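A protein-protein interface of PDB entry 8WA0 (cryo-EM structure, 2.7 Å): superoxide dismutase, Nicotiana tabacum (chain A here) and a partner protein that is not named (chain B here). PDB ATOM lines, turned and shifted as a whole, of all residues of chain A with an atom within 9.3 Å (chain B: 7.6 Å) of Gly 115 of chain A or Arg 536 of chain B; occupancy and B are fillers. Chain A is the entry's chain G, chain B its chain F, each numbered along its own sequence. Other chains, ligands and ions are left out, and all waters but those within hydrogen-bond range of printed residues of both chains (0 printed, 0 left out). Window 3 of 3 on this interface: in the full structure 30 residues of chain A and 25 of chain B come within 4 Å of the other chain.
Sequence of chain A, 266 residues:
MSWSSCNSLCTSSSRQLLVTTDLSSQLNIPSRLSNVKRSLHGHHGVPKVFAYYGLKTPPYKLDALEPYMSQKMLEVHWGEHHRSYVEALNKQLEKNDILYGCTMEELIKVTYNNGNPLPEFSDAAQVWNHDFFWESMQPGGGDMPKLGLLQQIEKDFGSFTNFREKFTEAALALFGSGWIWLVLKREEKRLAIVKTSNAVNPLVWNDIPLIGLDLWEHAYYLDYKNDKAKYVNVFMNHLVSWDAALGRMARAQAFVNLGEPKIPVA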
ATOM      1  N   ILE A 108     -10.674 -24.407 -24.770  1.00  0.00           N
ATOM      2  CA  ILE A 108     -10.786 -24.327 -23.368  1.00  0.00           C
ATOM      3  C   ILE A 108     -10.319 -25.607 -22.739  1.00  0.00           C
ATOM      4  O   ILE A 108      -9.507 -25.589 -21.820  1.00  0.00           O
ATOM      5  CB  ILE A 108     -12.209 -24.290 -22.992  1.00  0.00           C
ATOM      6  CG1 ILE A 108     -12.938 -23.156 -23.649  1.00  0.00           C
ATOM      7  CG2 ILE A 108     -12.307 -24.249 -21.490  1.00  0.00           C
ATOM      8  CD1 ILE A 108     -14.326 -23.624 -23.974  1.00  0.00           C
ATOM      9  N   LYS A 109     -10.768 -26.735 -23.250  1.00  0.00           N
ATOM     10  CA  LYS A 109     -10.385 -28.042 -22.721  1.00  0.00           C
ATOM     11  C   LYS A 109      -8.934 -28.436 -22.864  1.00  0.00           C
ATOM     12  O   LYS A 109      -8.392 -29.076 -21.996  1.00  0.00           O
ATOM     13  CB  LYS A 109     -11.309 -29.103 -23.255  1.00  0.00           C
ATOM     14  CG  LYS A 109     -11.297 -30.422 -22.507  1.00  0.00           C
ATOM     15  CD  LYS A 109     -12.211 -31.426 -23.192  1.00  0.00           C
ATOM     16  CE  LYS A 109     -12.163 -32.786 -22.516  1.00  0.00           C
ATOM     17  NZ  LYS A 109     -12.731 -32.753 -21.142  1.00  0.00           N
ATOM     18  N   VAL A 110      -8.304 -28.093 -23.956  1.00  0.00           N
ATOM     19  CA  VAL A 110      -6.901 -28.381 -24.131  1.00  0.00           C
ATOM     20  C   VAL A 110      -6.059 -27.626 -23.166  1.00  0.00           C
ATOM     21  O   VAL A 110      -5.160 -28.164 -22.545  1.00  0.00           O
ATOM     22  CB  VAL A 110      -6.456 -28.040 -25.547  1.00  0.00           C
ATOM     23  CG1 VAL A 110      -4.960 -27.789 -25.632  1.00  0.00           C
ATOM     24  CG2 VAL A 110      -6.854 -29.148 -26.506  1.00  0.00           C
ATOM     25  N   THR A 111      -6.393 -26.372 -22.990  1.00  0.00           N
ATOM     26  CA  THR A 111      -5.649 -25.525 -22.115  1.00  0.00           C
ATOM     27  C   THR A 111      -5.677 -25.898 -20.630  1.00  0.00           C
ATOM     28  O   THR A 111      -4.687 -25.716 -19.953  1.00  0.00           O
ATOM     29  CB  THR A 111      -6.026 -24.089 -22.414  1.00  0.00           C
ATOM     30  OG1 THR A 111      -7.440 -23.940 -22.358  1.00  0.00           O
ATOM     31  CG2 THR A 111      -5.540 -23.695 -23.785  1.00  0.00           C
ATOM     32  N   TYR A 112      -6.769 -26.422 -20.115  1.00  0.00           N
ATOM     33  CA  TYR A 112      -6.875 -26.801 -18.727  1.00  0.00           C
ATOM     34  C   TYR A 112      -5.847 -27.819 -18.323  1.00  0.00           C
ATOM     35  O   TYR A 112      -5.425 -27.803 -17.181  1.00  0.00           O
ATOM     36  CB  TYR A 112      -8.284 -27.213 -18.421  1.00  0.00           C
ATOM     37  CG  TYR A 112      -8.652 -27.675 -17.057  1.00  0.00           C
ATOM     38  CD1 TYR A 112      -8.955 -26.774 -16.071  1.00  0.00           C
ATOM     39  CD2 TYR A 112      -8.810 -29.016 -16.784  1.00  0.00           C
ATOM     40  CE1 TYR A 112      -9.335 -27.195 -14.823  1.00  0.00           C
ATOM     41  CE2 TYR A 112      -9.197 -29.446 -15.533  1.00  0.00           C
ATOM     42  CZ  TYR A 112      -9.461 -28.521 -14.558  1.00  0.00           C
ATOM     43  OH  TYR A 112      -9.846 -28.913 -13.301  1.00  0.00           O
ATOM     44  N   ASN A 113      -5.444 -28.722 -19.177  1.00  0.00           N
ATOM     45  CA  ASN A 113      -4.368 -29.657 -18.862  1.00  0.00           C
ATOM     46  C   ASN A 113      -4.574 -30.379 -17.566  1.00  0.00           C
ATOM     47  O   ASN A 113      -3.666 -30.484 -16.768  1.00  0.00           O
ATOM     48  CB  ASN A 113      -3.004 -29.032 -18.974  1.00  0.00           C
ATOM     49  CG  ASN A 113      -1.915 -30.043 -19.204  1.00  0.00           C
ATOM     50  OD1 ASN A 113      -2.160 -31.117 -19.736  1.00  0.00           O
ATOM     51  ND2 ASN A 113      -0.699 -29.699 -18.808  1.00  0.00           N
ATOM     52  N   ASN A 114      -5.775 -30.839 -17.326  1.00  0.00           N
ATOM     53  CA  ASN A 114      -6.089 -31.599 -16.149  1.00  0.00           C
ATOM     54  C   ASN A 114      -5.616 -30.963 -14.898  1.00  0.00           C
ATOM     55  O   ASN A 114      -4.923 -31.584 -14.101  1.00  0.00           O
ATOM     56  CB  ASN A 114      -5.658 -33.029 -16.277  1.00  0.00           C
ATOM     57  CG  ASN A 114      -6.608 -33.984 -15.599  1.00  0.00           C
ATOM     58  OD1 ASN A 114      -7.748 -33.637 -15.312  1.00  0.00           O
ATOM     59  ND2 ASN A 114      -6.146 -35.200 -15.349  1.00  0.00           N
ATOM     60  N   GLY A 115      -5.975 -29.721 -14.704  1.00  0.00           N
ATOM     61  CA  GLY A 115      -5.580 -29.015 -13.514  1.00  0.00           C
ATOM     62  C   GLY A 115      -4.329 -28.180 -13.475  1.00  0.00           C
ATOM     63  O   GLY A 115      -3.982 -27.675 -12.415  1.00  0.00           O
ATOM     64  N   ASN A 116      -3.641 -28.013 -14.584  1.00  0.00           N
ATOM     65  CA  ASN A 116      -2.499 -27.127 -14.604  1.00  0.00           C
ATOM     66  C   ASN A 116      -2.673 -26.221 -15.753  1.00  0.00           C
ATOM     67  O   ASN A 116      -1.980 -26.334 -16.740  1.00  0.00           O
ATOM     68  CB  ASN A 116      -1.203 -27.880 -14.765  1.00  0.00           C
ATOM     69  CG  ASN A 116       0.003 -27.057 -14.356  1.00  0.00           C
ATOM     70  OD1 ASN A 116       1.085 -27.188 -14.929  1.00  0.00           O
ATOM     71  ND2 ASN A 116      -0.182 -26.191 -13.366  1.00  0.00           N
ATOM     72  N   PRO A 117      -3.552 -25.266 -15.597  1.00  0.00           N
ATOM     73  CA  PRO A 117      -3.769 -24.501 -16.778  1.00  0.00           C
ATOM     74  C   PRO A 117      -2.587 -23.921 -17.454  1.00  0.00           C
ATOM     75  O   PRO A 117      -1.697 -23.385 -16.840  1.00  0.00           O
ATOM     76  CB  PRO A 117      -4.677 -23.429 -16.284  1.00  0.00           C
ATOM     77  CG  PRO A 117      -5.559 -24.133 -15.331  1.00  0.00           C
ATOM     78  CD  PRO A 117      -4.629 -25.057 -14.618  1.00  0.00           C
ATOM     79  N   LEU A 118      -2.592 -24.028 -18.752  1.00  0.00           N
ATOM     80  CA  LEU A 118      -1.546 -23.547 -19.560  1.00  0.00           C
ATOM     81  C   LEU A 118      -1.702 -22.083 -19.609  1.00  0.00           C
ATOM     82  O   LEU A 118      -2.710 -21.559 -19.178  1.00  0.00           O
ATOM     83  CB  LEU A 118      -1.728 -24.116 -20.955  1.00  0.00           C
ATOM     84  CG  LEU A 118      -1.611 -25.607 -21.255  1.00  0.00           C
ATOM     85  CD1 LEU A 118      -1.935 -25.865 -22.716  1.00  0.00           C
ATOM     86  CD2 LEU A 118      -0.236 -26.143 -20.923  1.00  0.00           C
ATOM     87  N   PHE A 121      -5.174 -20.220 -20.881  1.00  0.00           N
ATOM     88  CA  PHE A 121      -6.530 -20.610 -20.478  1.00  0.00           C
ATOM     89  C   PHE A 121      -7.489 -19.487 -20.177  1.00  0.00           C
ATOM     90  O   PHE A 121      -8.622 -19.400 -20.743  1.00  0.00           O
ATOM     91  CB  PHE A 121      -6.428 -21.501 -19.239  1.00  0.00           C
ATOM     92  CG  PHE A 121      -7.749 -21.970 -18.704  1.00  0.00           C
ATOM     93  CD1 PHE A 121      -8.463 -22.955 -19.356  1.00  0.00           C
ATOM     94  CD2 PHE A 121      -8.259 -21.448 -17.530  1.00  0.00           C
ATOM     95  CE1 PHE A 121      -9.672 -23.396 -18.860  1.00  0.00           C
ATOM     96  CE2 PHE A 121      -9.467 -21.884 -17.029  1.00  0.00           C
ATOM     97  CZ  PHE A 121     -10.175 -22.861 -17.695  1.00  0.00           C
ATOM     98  N   SER A 197     -15.137 -21.484  -9.235  1.00  0.00           N
ATOM     99  CA  SER A 197     -14.386 -20.328  -8.873  1.00  0.00           C
ATOM    100  C   SER A 197     -13.656 -19.828 -10.037  1.00  0.00           C
ATOM    101  O   SER A 197     -13.202 -20.602 -10.862  1.00  0.00           O
ATOM    102  CB  SER A 197     -13.370 -20.721  -7.844  1.00  0.00           C
ATOM    103  OG  SER A 197     -12.518 -21.732  -8.344  1.00  0.00           O
ATOM    104  N   VAL A 200     -12.983 -21.053 -14.702  1.00  0.00           N
ATOM    105  CA  VAL A 200     -13.440 -22.313 -15.178  1.00  0.00           C
ATOM    106  C   VAL A 200     -14.924 -22.378 -15.531  1.00  0.00           C
ATOM    107  O   VAL A 200     -15.755 -21.926 -14.765  1.00  0.00           O
ATOM    108  CB  VAL A 200     -13.051 -23.316 -14.096  1.00  0.00           C
ATOM    109  CG1 VAL A 200     -13.694 -24.669 -14.328  1.00  0.00           C
ATOM    110  CG2 VAL A 200     -11.546 -23.434 -14.012  1.00  0.00           C
ATOM    111  N   VAL A 204     -15.238 -27.805 -19.083  1.00  0.00           N
ATOM    112  CA  VAL A 204     -14.028 -28.541 -18.796  1.00  0.00           C
ATOM    113  C   VAL A 204     -14.243 -29.945 -18.241  1.00  0.00           C
ATOM    114  O   VAL A 204     -13.363 -30.775 -18.336  1.00  0.00           O
ATOM    115  CB  VAL A 204     -13.100 -27.727 -17.912  1.00  0.00           C
ATOM    116  CG1 VAL A 204     -12.731 -26.427 -18.578  1.00  0.00           C
ATOM    117  CG2 VAL A 204     -13.741 -27.473 -16.567  1.00  0.00           C
ATOM    118  N   TRP A 205     -15.382 -30.208 -17.629  1.00  0.00           N
ATOM    119  CA  TRP A 205     -15.681 -31.520 -17.104  1.00  0.00           C
ATOM    120  C   TRP A 205     -16.768 -32.211 -17.926  1.00  0.00           C
ATOM    121  O   TRP A 205     -17.492 -33.046 -17.405  1.00  0.00           O
ATOM    122  CB  TRP A 205     -16.128 -31.461 -15.669  1.00  0.00           C
ATOM    123  CG  TRP A 205     -15.250 -30.751 -14.738  1.00  0.00           C
ATOM    124  CD1 TRP A 205     -13.984 -31.086 -14.389  1.00  0.00           C
ATOM    125  CD2 TRP A 205     -15.589 -29.597 -13.975  1.00  0.00           C
ATOM    126  NE1 TRP A 205     -13.497 -30.191 -13.473  1.00  0.00           N
ATOM    127  CE2 TRP A 205     -14.468 -29.265 -13.204  1.00  0.00           C
ATOM    128  CE3 TRP A 205     -16.730 -28.800 -13.887  1.00  0.00           C
ATOM    129  CZ2 TRP A 205     -14.452 -28.173 -12.352  1.00  0.00           C
ATOM    130  CZ3 TRP A 205     -16.714 -27.722 -13.047  1.00  0.00           C
ATOM    131  CH2 TRP A 205     -15.584 -27.414 -12.285  1.00  0.00           C
ATOM    132  N   MET B 529       5.667 -25.903  -2.423  1.00  0.00           N
ATOM    133  CA  MET B 529       4.588 -26.803  -2.409  1.00  0.00           C
ATOM    134  C   MET B 529       3.631 -26.269  -1.436  1.00  0.00           C
ATOM    135  O   MET B 529       2.442 -26.304  -1.669  1.00  0.00           O
ATOM    136  CB  MET B 529       5.079 -28.151  -1.930  1.00  0.00           C
ATOM    137  CG  MET B 529       4.043 -29.259  -1.957  1.00  0.00           C
ATOM    138  SD  MET B 529       4.634 -30.744  -1.122  1.00  0.00           S
ATOM    139  CE  MET B 529       6.210 -30.985  -1.938  1.00  0.00           C
ATOM    140  N   LEU B 530       4.122 -25.767  -0.327  1.00  0.00           N
ATOM    141  CA  LEU B 530       3.222 -25.337   0.712  1.00  0.00           C
ATOM    142  C   LEU B 530       2.427 -24.216   0.206  1.00  0.00           C
ATOM    143  O   LEU B 530       1.240 -24.112   0.459  1.00  0.00           O
ATOM    144  CB  LEU B 530       3.971 -24.973   1.967  1.00  0.00           C
ATOM    145  CG  LEU B 530       4.623 -26.151   2.684  1.00  0.00           C
ATOM    146  CD1 LEU B 530       5.498 -25.674   3.831  1.00  0.00           C
ATOM    147  CD2 LEU B 530       3.568 -27.131   3.168  1.00  0.00           C
ATOM    148  N   ARG B 531       3.078 -23.382  -0.551  1.00  0.00           N
ATOM    149  CA  ARG B 531       2.393 -22.273  -1.115  1.00  0.00           C
ATOM    150  C   ARG B 531       1.293 -22.733  -2.076  1.00  0.00           C
ATOM    151  O   ARG B 531       0.200 -22.192  -2.062  1.00  0.00           O
ATOM    152  CB  ARG B 531       3.420 -21.363  -1.744  1.00  0.00           C
ATOM    153  CG  ARG B 531       2.929 -19.990  -2.143  1.00  0.00           C
ATOM    154  CD  ARG B 531       4.033 -19.326  -2.933  1.00  0.00           C
ATOM    155  NE  ARG B 531       5.333 -19.755  -2.429  1.00  0.00           N
ATOM    156  CZ  ARG B 531       6.484 -19.521  -3.042  1.00  0.00           C
ATOM    157  NH1 ARG B 531       6.500 -18.859  -4.189  1.00  0.00           N
ATOM    158  NH2 ARG B 531       7.619 -19.951  -2.511  1.00  0.00           N
ATOM    159  N   ASP B 532       1.556 -23.733  -2.902  1.00  0.00           N
ATOM    160  CA  ASP B 532       0.558 -24.293  -3.811  1.00  0.00           C
ATOM    161  C   ASP B 532      -0.576 -24.949  -3.137  1.00  0.00           C
ATOM    162  O   ASP B 532      -1.681 -24.849  -3.599  1.00  0.00           O
ATOM    163  CB  ASP B 532       1.212 -25.407  -4.587  1.00  0.00           C
ATOM    164  CG  ASP B 532       0.295 -26.036  -5.605  1.00  0.00           C
ATOM    165  OD1 ASP B 532      -0.421 -25.292  -6.297  1.00  0.00           O
ATOM    166  OD2 ASP B 532       0.302 -27.279  -5.723  1.00  0.00           O
ATOM    167  N   ILE B 533      -0.335 -25.661  -2.054  1.00  0.00           N
ATOM    168  CA  ILE B 533      -1.382 -26.436  -1.462  1.00  0.00           C
ATOM    169  C   ILE B 533      -2.397 -25.475  -1.153  1.00  0.00           C
ATOM    170  O   ILE B 533      -3.566 -25.678  -1.406  1.00  0.00           O
ATOM    171  CB  ILE B 533      -0.964 -27.050  -0.150  1.00  0.00           C
ATOM    172  CG1 ILE B 533       0.194 -28.021  -0.359  1.00  0.00           C
ATOM    173  CG2 ILE B 533      -2.125 -27.790   0.487  1.00  0.00           C
ATOM    174  CD1 ILE B 533      -0.135 -29.184  -1.266  1.00  0.00           C
ATOM    175  N   SER B 534      -1.987 -24.369  -0.558  1.00  0.00           N
ATOM    176  CA  SER B 534      -2.960 -23.397  -0.110  1.00  0.00           C
ATOM    177  C   SER B 534      -3.606 -22.685  -1.263  1.00  0.00           C
ATOM    178  O   SER B 534      -4.806 -22.429  -1.249  1.00  0.00           O
ATOM    179  CB  SER B 534      -2.299 -22.397   0.823  1.00  0.00           C
ATOM    180  OG  SER B 534      -1.033 -22.017   0.325  1.00  0.00           O
ATOM    181  N   CYS B 535      -2.814 -22.372  -2.276  1.00  0.00           N
ATOM    182  CA  CYS B 535      -3.352 -21.650  -3.403  1.00  0.00           C
ATOM    183  C   CYS B 535      -4.420 -22.489  -4.052  1.00  0.00           C
ATOM    184  O   CYS B 535      -5.491 -21.996  -4.376  1.00  0.00           O
ATOM    185  CB  CYS B 535      -2.255 -21.366  -4.419  1.00  0.00           C
ATOM    186  SG  CYS B 535      -1.208 -19.948  -4.023  1.00  0.00           S
ATOM    187  N   ARG B 536      -4.150 -23.774  -4.204  1.00  0.00           N
ATOM    188  CA  ARG B 536      -5.102 -24.645  -4.851  1.00  0.00           C
ATOM    189  C   ARG B 536      -6.301 -24.855  -3.968  1.00  0.00           C
ATOM    190  O   ARG B 536      -7.433 -24.817  -4.443  1.00  0.00           O
ATOM    191  CB  ARG B 536      -4.462 -25.981  -5.207  1.00  0.00           C
ATOM    192  CG  ARG B 536      -3.861 -26.008  -6.602  1.00  0.00           C
ATOM    193  CD  ARG B 536      -3.379 -27.398  -6.981  1.00  0.00           C
ATOM    194  NE  ARG B 536      -3.227 -27.550  -8.426  1.00  0.00           N
ATOM    195  CZ  ARG B 536      -2.091 -27.354  -9.091  1.00  0.00           C
ATOM    196  NH1 ARG B 536      -0.991 -27.006  -8.447  1.00  0.00           N
ATOM    197  NH2 ARG B 536      -2.051 -27.515 -10.403  1.00  0.00           N
ATOM    198  N   ARG B 537      -6.071 -25.053  -2.677  1.00  0.00           N
ATOM    199  CA  ARG B 537      -7.170 -25.327  -1.794  1.00  0.00           C
ATOM    200  C   ARG B 537      -8.209 -24.255  -1.736  1.00  0.00           C
ATOM    201  O   ARG B 537      -9.347 -24.510  -1.368  1.00  0.00           O
ATOM    202  CB  ARG B 537      -6.695 -25.720  -0.429  1.00  0.00           C
ATOM    203  CG  ARG B 537      -6.331 -27.184  -0.313  1.00  0.00           C
ATOM    204  CD  ARG B 537      -7.566 -28.054  -0.451  1.00  0.00           C
ATOM    205  NE  ARG B 537      -8.580 -27.710   0.541  1.00  0.00           N
ATOM    206  CZ  ARG B 537      -9.746 -28.334   0.660  1.00  0.00           C
ATOM    207  NH1 ARG B 537     -10.047 -29.339  -0.151  1.00  0.00           N
ATOM    208  NH2 ARG B 537     -10.614 -27.955   1.587  1.00  0.00           N
ATOM    209  N   ALA B 538      -7.834 -23.033  -2.087  1.00  0.00           N
ATOM    210  CA  ALA B 538      -8.768 -21.919  -2.037  1.00  0.00           C
ATOM    211  C   ALA B 538      -9.312 -21.620  -3.411  1.00  0.00           C
ATOM    212  O   ALA B 538     -10.378 -21.028  -3.555  1.00  0.00           O
ATOM    213  CB  ALA B 538      -8.084 -20.692  -1.476  1.00  0.00           C
ATOM    214  N   LEU B 539      -8.579 -22.037  -4.430  1.00  0.00           N
ATOM    215  CA  LEU B 539      -9.006 -21.779  -5.793  1.00  0.00           C
ATOM    216  C   LEU B 539      -9.884 -22.890  -6.349  1.00  0.00           C
ATOM    217  O   LEU B 539     -10.287 -22.833  -7.504  1.00  0.00           O
ATOM    218  CB  LEU B 539      -7.798 -21.547  -6.691  1.00  0.00           C
ATOM    219  CG  LEU B 539      -7.172 -20.164  -6.554  1.00  0.00           C
ATOM    220  CD1 LEU B 539      -5.901 -20.065  -7.380  1.00  0.00           C
ATOM    221  CD2 LEU B 539      -8.177 -19.103  -6.969  1.00  0.00           C
ATOM    222  N   GLY B 540     -10.162 -23.913  -5.549  1.00  0.00           N
ATOM    223  CA  GLY B 540     -11.035 -24.986  -5.990  1.00  0.00           C
ATOM    224  C   GLY B 540     -10.441 -25.733  -7.157  1.00  0.00           C
ATOM    225  O   GLY B 540     -11.112 -25.956  -8.160  1.00  0.00           O
ATOM    226  N   LEU B 541      -9.186 -26.130  -7.037  1.00  0.00           N
ATOM    227  CA  LEU B 541      -8.516 -26.824  -8.103  1.00  0.00           C
ATOM    228  C   LEU B 541      -8.056 -28.189  -7.649  1.00  0.00           C
ATOM    229  O   LEU B 541      -8.189 -28.512  -6.494  1.00  0.00           O
ATOM    230  CB  LEU B 541      -7.381 -25.973  -8.639  1.00  0.00           C
ATOM    231  N   PRO B 542      -7.596 -29.031  -8.576  1.00  0.00           N
ATOM    232  CA  PRO B 542      -7.262 -30.405  -8.217  1.00  0.00           C
ATOM    233  C   PRO B 542      -5.971 -30.683  -7.525  1.00  0.00           C
ATOM    234  O   PRO B 542      -4.930 -30.288  -8.012  1.00  0.00           O
ATOM    235  CB  PRO B 542      -7.219 -31.079  -9.561  1.00  0.00           C
ATOM    236  CG  PRO B 542      -8.153 -30.308 -10.406  1.00  0.00           C
ATOM    237  CD  PRO B 542      -7.812 -28.913 -10.027  1.00  0.00           C
ATOM    238  N   LEU B 543      -6.040 -31.348  -6.390  1.00  0.00           N
ATOM    239  CA  LEU B 543      -4.868 -31.656  -5.630  1.00  0.00           C
ATOM    240  C   LEU B 543      -3.916 -32.692  -6.164  1.00  0.00           C
ATOM    241  O   LEU B 543      -2.707 -32.493  -6.130  1.00  0.00           O
ATOM    242  CB  LEU B 543      -5.290 -32.031  -4.239  1.00  0.00           C
ATOM    243  CG  LEU B 543      -5.859 -30.884  -3.401  1.00  0.00           C
ATOM    244  CD1 LEU B 543      -6.310 -31.396  -2.042  1.00  0.00           C
ATOM    245  CD2 LEU B 543      -4.835 -29.772  -3.244  1.00  0.00           C
ATOM    246  N   GLU B 544      -4.437 -33.799  -6.668  1.00  0.00           N
ATOM    247  CA  GLU B 544      -3.607 -34.885  -7.163  1.00  0.00           C
ATOM    248  C   GLU B 544      -4.163 -35.146  -8.536  1.00  0.00           C
ATOM    249  O   GLU B 544      -5.224 -34.633  -8.840  1.00  0.00           O
ATOM    250  CB  GLU B 544      -3.676 -36.066  -6.225  1.00  0.00           C
ATOM    251  CG  GLU B 544      -2.843 -37.272  -6.625  1.00  0.00           C
ATOM    252  CD  GLU B 544      -1.374 -36.951  -6.819  1.00  0.00           C
ATOM    253  OE1 GLU B 544      -0.803 -36.206  -5.996  1.00  0.00           O
ATOM    254  OE2 GLU B 544      -0.785 -37.461  -7.795  1.00  0.00           O
ATOM    255  N   PRO B 546      -6.087 -35.811 -11.624  1.00  0.00           N
ATOM    256  CA  PRO B 546      -7.384 -36.458 -11.702  1.00  0.00           C
ATOM    257  C   PRO B 546      -7.229 -37.810 -12.397  1.00  0.00           C
ATOM    258  O   PRO B 546      -6.919 -37.848 -13.583  1.00  0.00           O
ATOM    259  CB  PRO B 546      -8.198 -35.480 -12.526  1.00  0.00           C
ATOM    260  CG  PRO B 546      -7.667 -34.162 -12.101  1.00  0.00           C
ATOM    261  CD  PRO B 546      -6.190 -34.404 -12.092  1.00  0.00           C
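The backbone carbonyl oxygen (O) of Pro 546 of chain B lies within hydrogen-bond range of the side-chain amide nitrogen (ND2) of Asn 114 of chain A. The backbone carbonyl oxygen of Leu 539 of chain B is in hydrogen-bond range of the side-chain hydroxyl of Ser 197 of chain A (2.6 Å). O of Gly 115 of chain A sits at hydrogen-bond distance from NH2 of Arg 536 of chain B.
Arg 536 of chain B touches just these residues of chain A: Gly 115 (2.8 Å) and Asn 116 (3.7 Å). No residue of chain A comes within 4 Å of Ala 538 of chain B. No residue of chain A comes within 4 Å of Leu 541 of chain B. Of chain A, only Tyr 112 comes within 4 Å of Pro 542 of chain B. Of the printed residues of chain A, Leu 539 of chain B touches Ser 197 (2.6 Å). Printed residues of chain B within 4 Å of Ser 197 of chain A: Leu 539. Of the printed residues of chain B, Asn 116 of chain A touches Arg 536 (3.7 Å). Asn 113 of chain A touches none of the printed residues of chain B. Thr 111 of chain A touches none of the printed residues of chain B. The nearest residue of chain A that does not touch Arg 536 of chain B is Pro 117 of chain A (5.5 Å). The nearest printed residue of chain B that does not touch Asn 116 of chain A is Pro 542 of chain B (6.2 Å).
Of the 17 printed residues of chain B, 4 touch a printed residue of chain A. Printed residues of chain B that touch a printed residue of chain A: Arg 536, Leu 539, Pro 542 and Pro 546. Of the 16 printed residues of chain A, 5 touch a printed residue of chain B. Among the printed residues, 5 pairs touch across the chains.
The side-chain carboxylate of Asp 532 of chain B lies within salt-bridge range of the guanidinium group of Arg 536 of chain B (2.8 Å). The backbone carbonyl oxygen of Arg 536 of chain B lies within hydrogen-bond range of the backbone NH of Leu 541 of chain B (3.4 Å). NE of Arg 536 of chain B is in hydrogen-bond range of O of Pro 542 of chain B (3.3 Å).
Among the printed residues, merely in contact across the chains: Tyr 112 of chain A with Pro 542 of chain B (3.6 Å) and Asn 116 of chain A with Arg 536 of chain B (3.7 Å).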
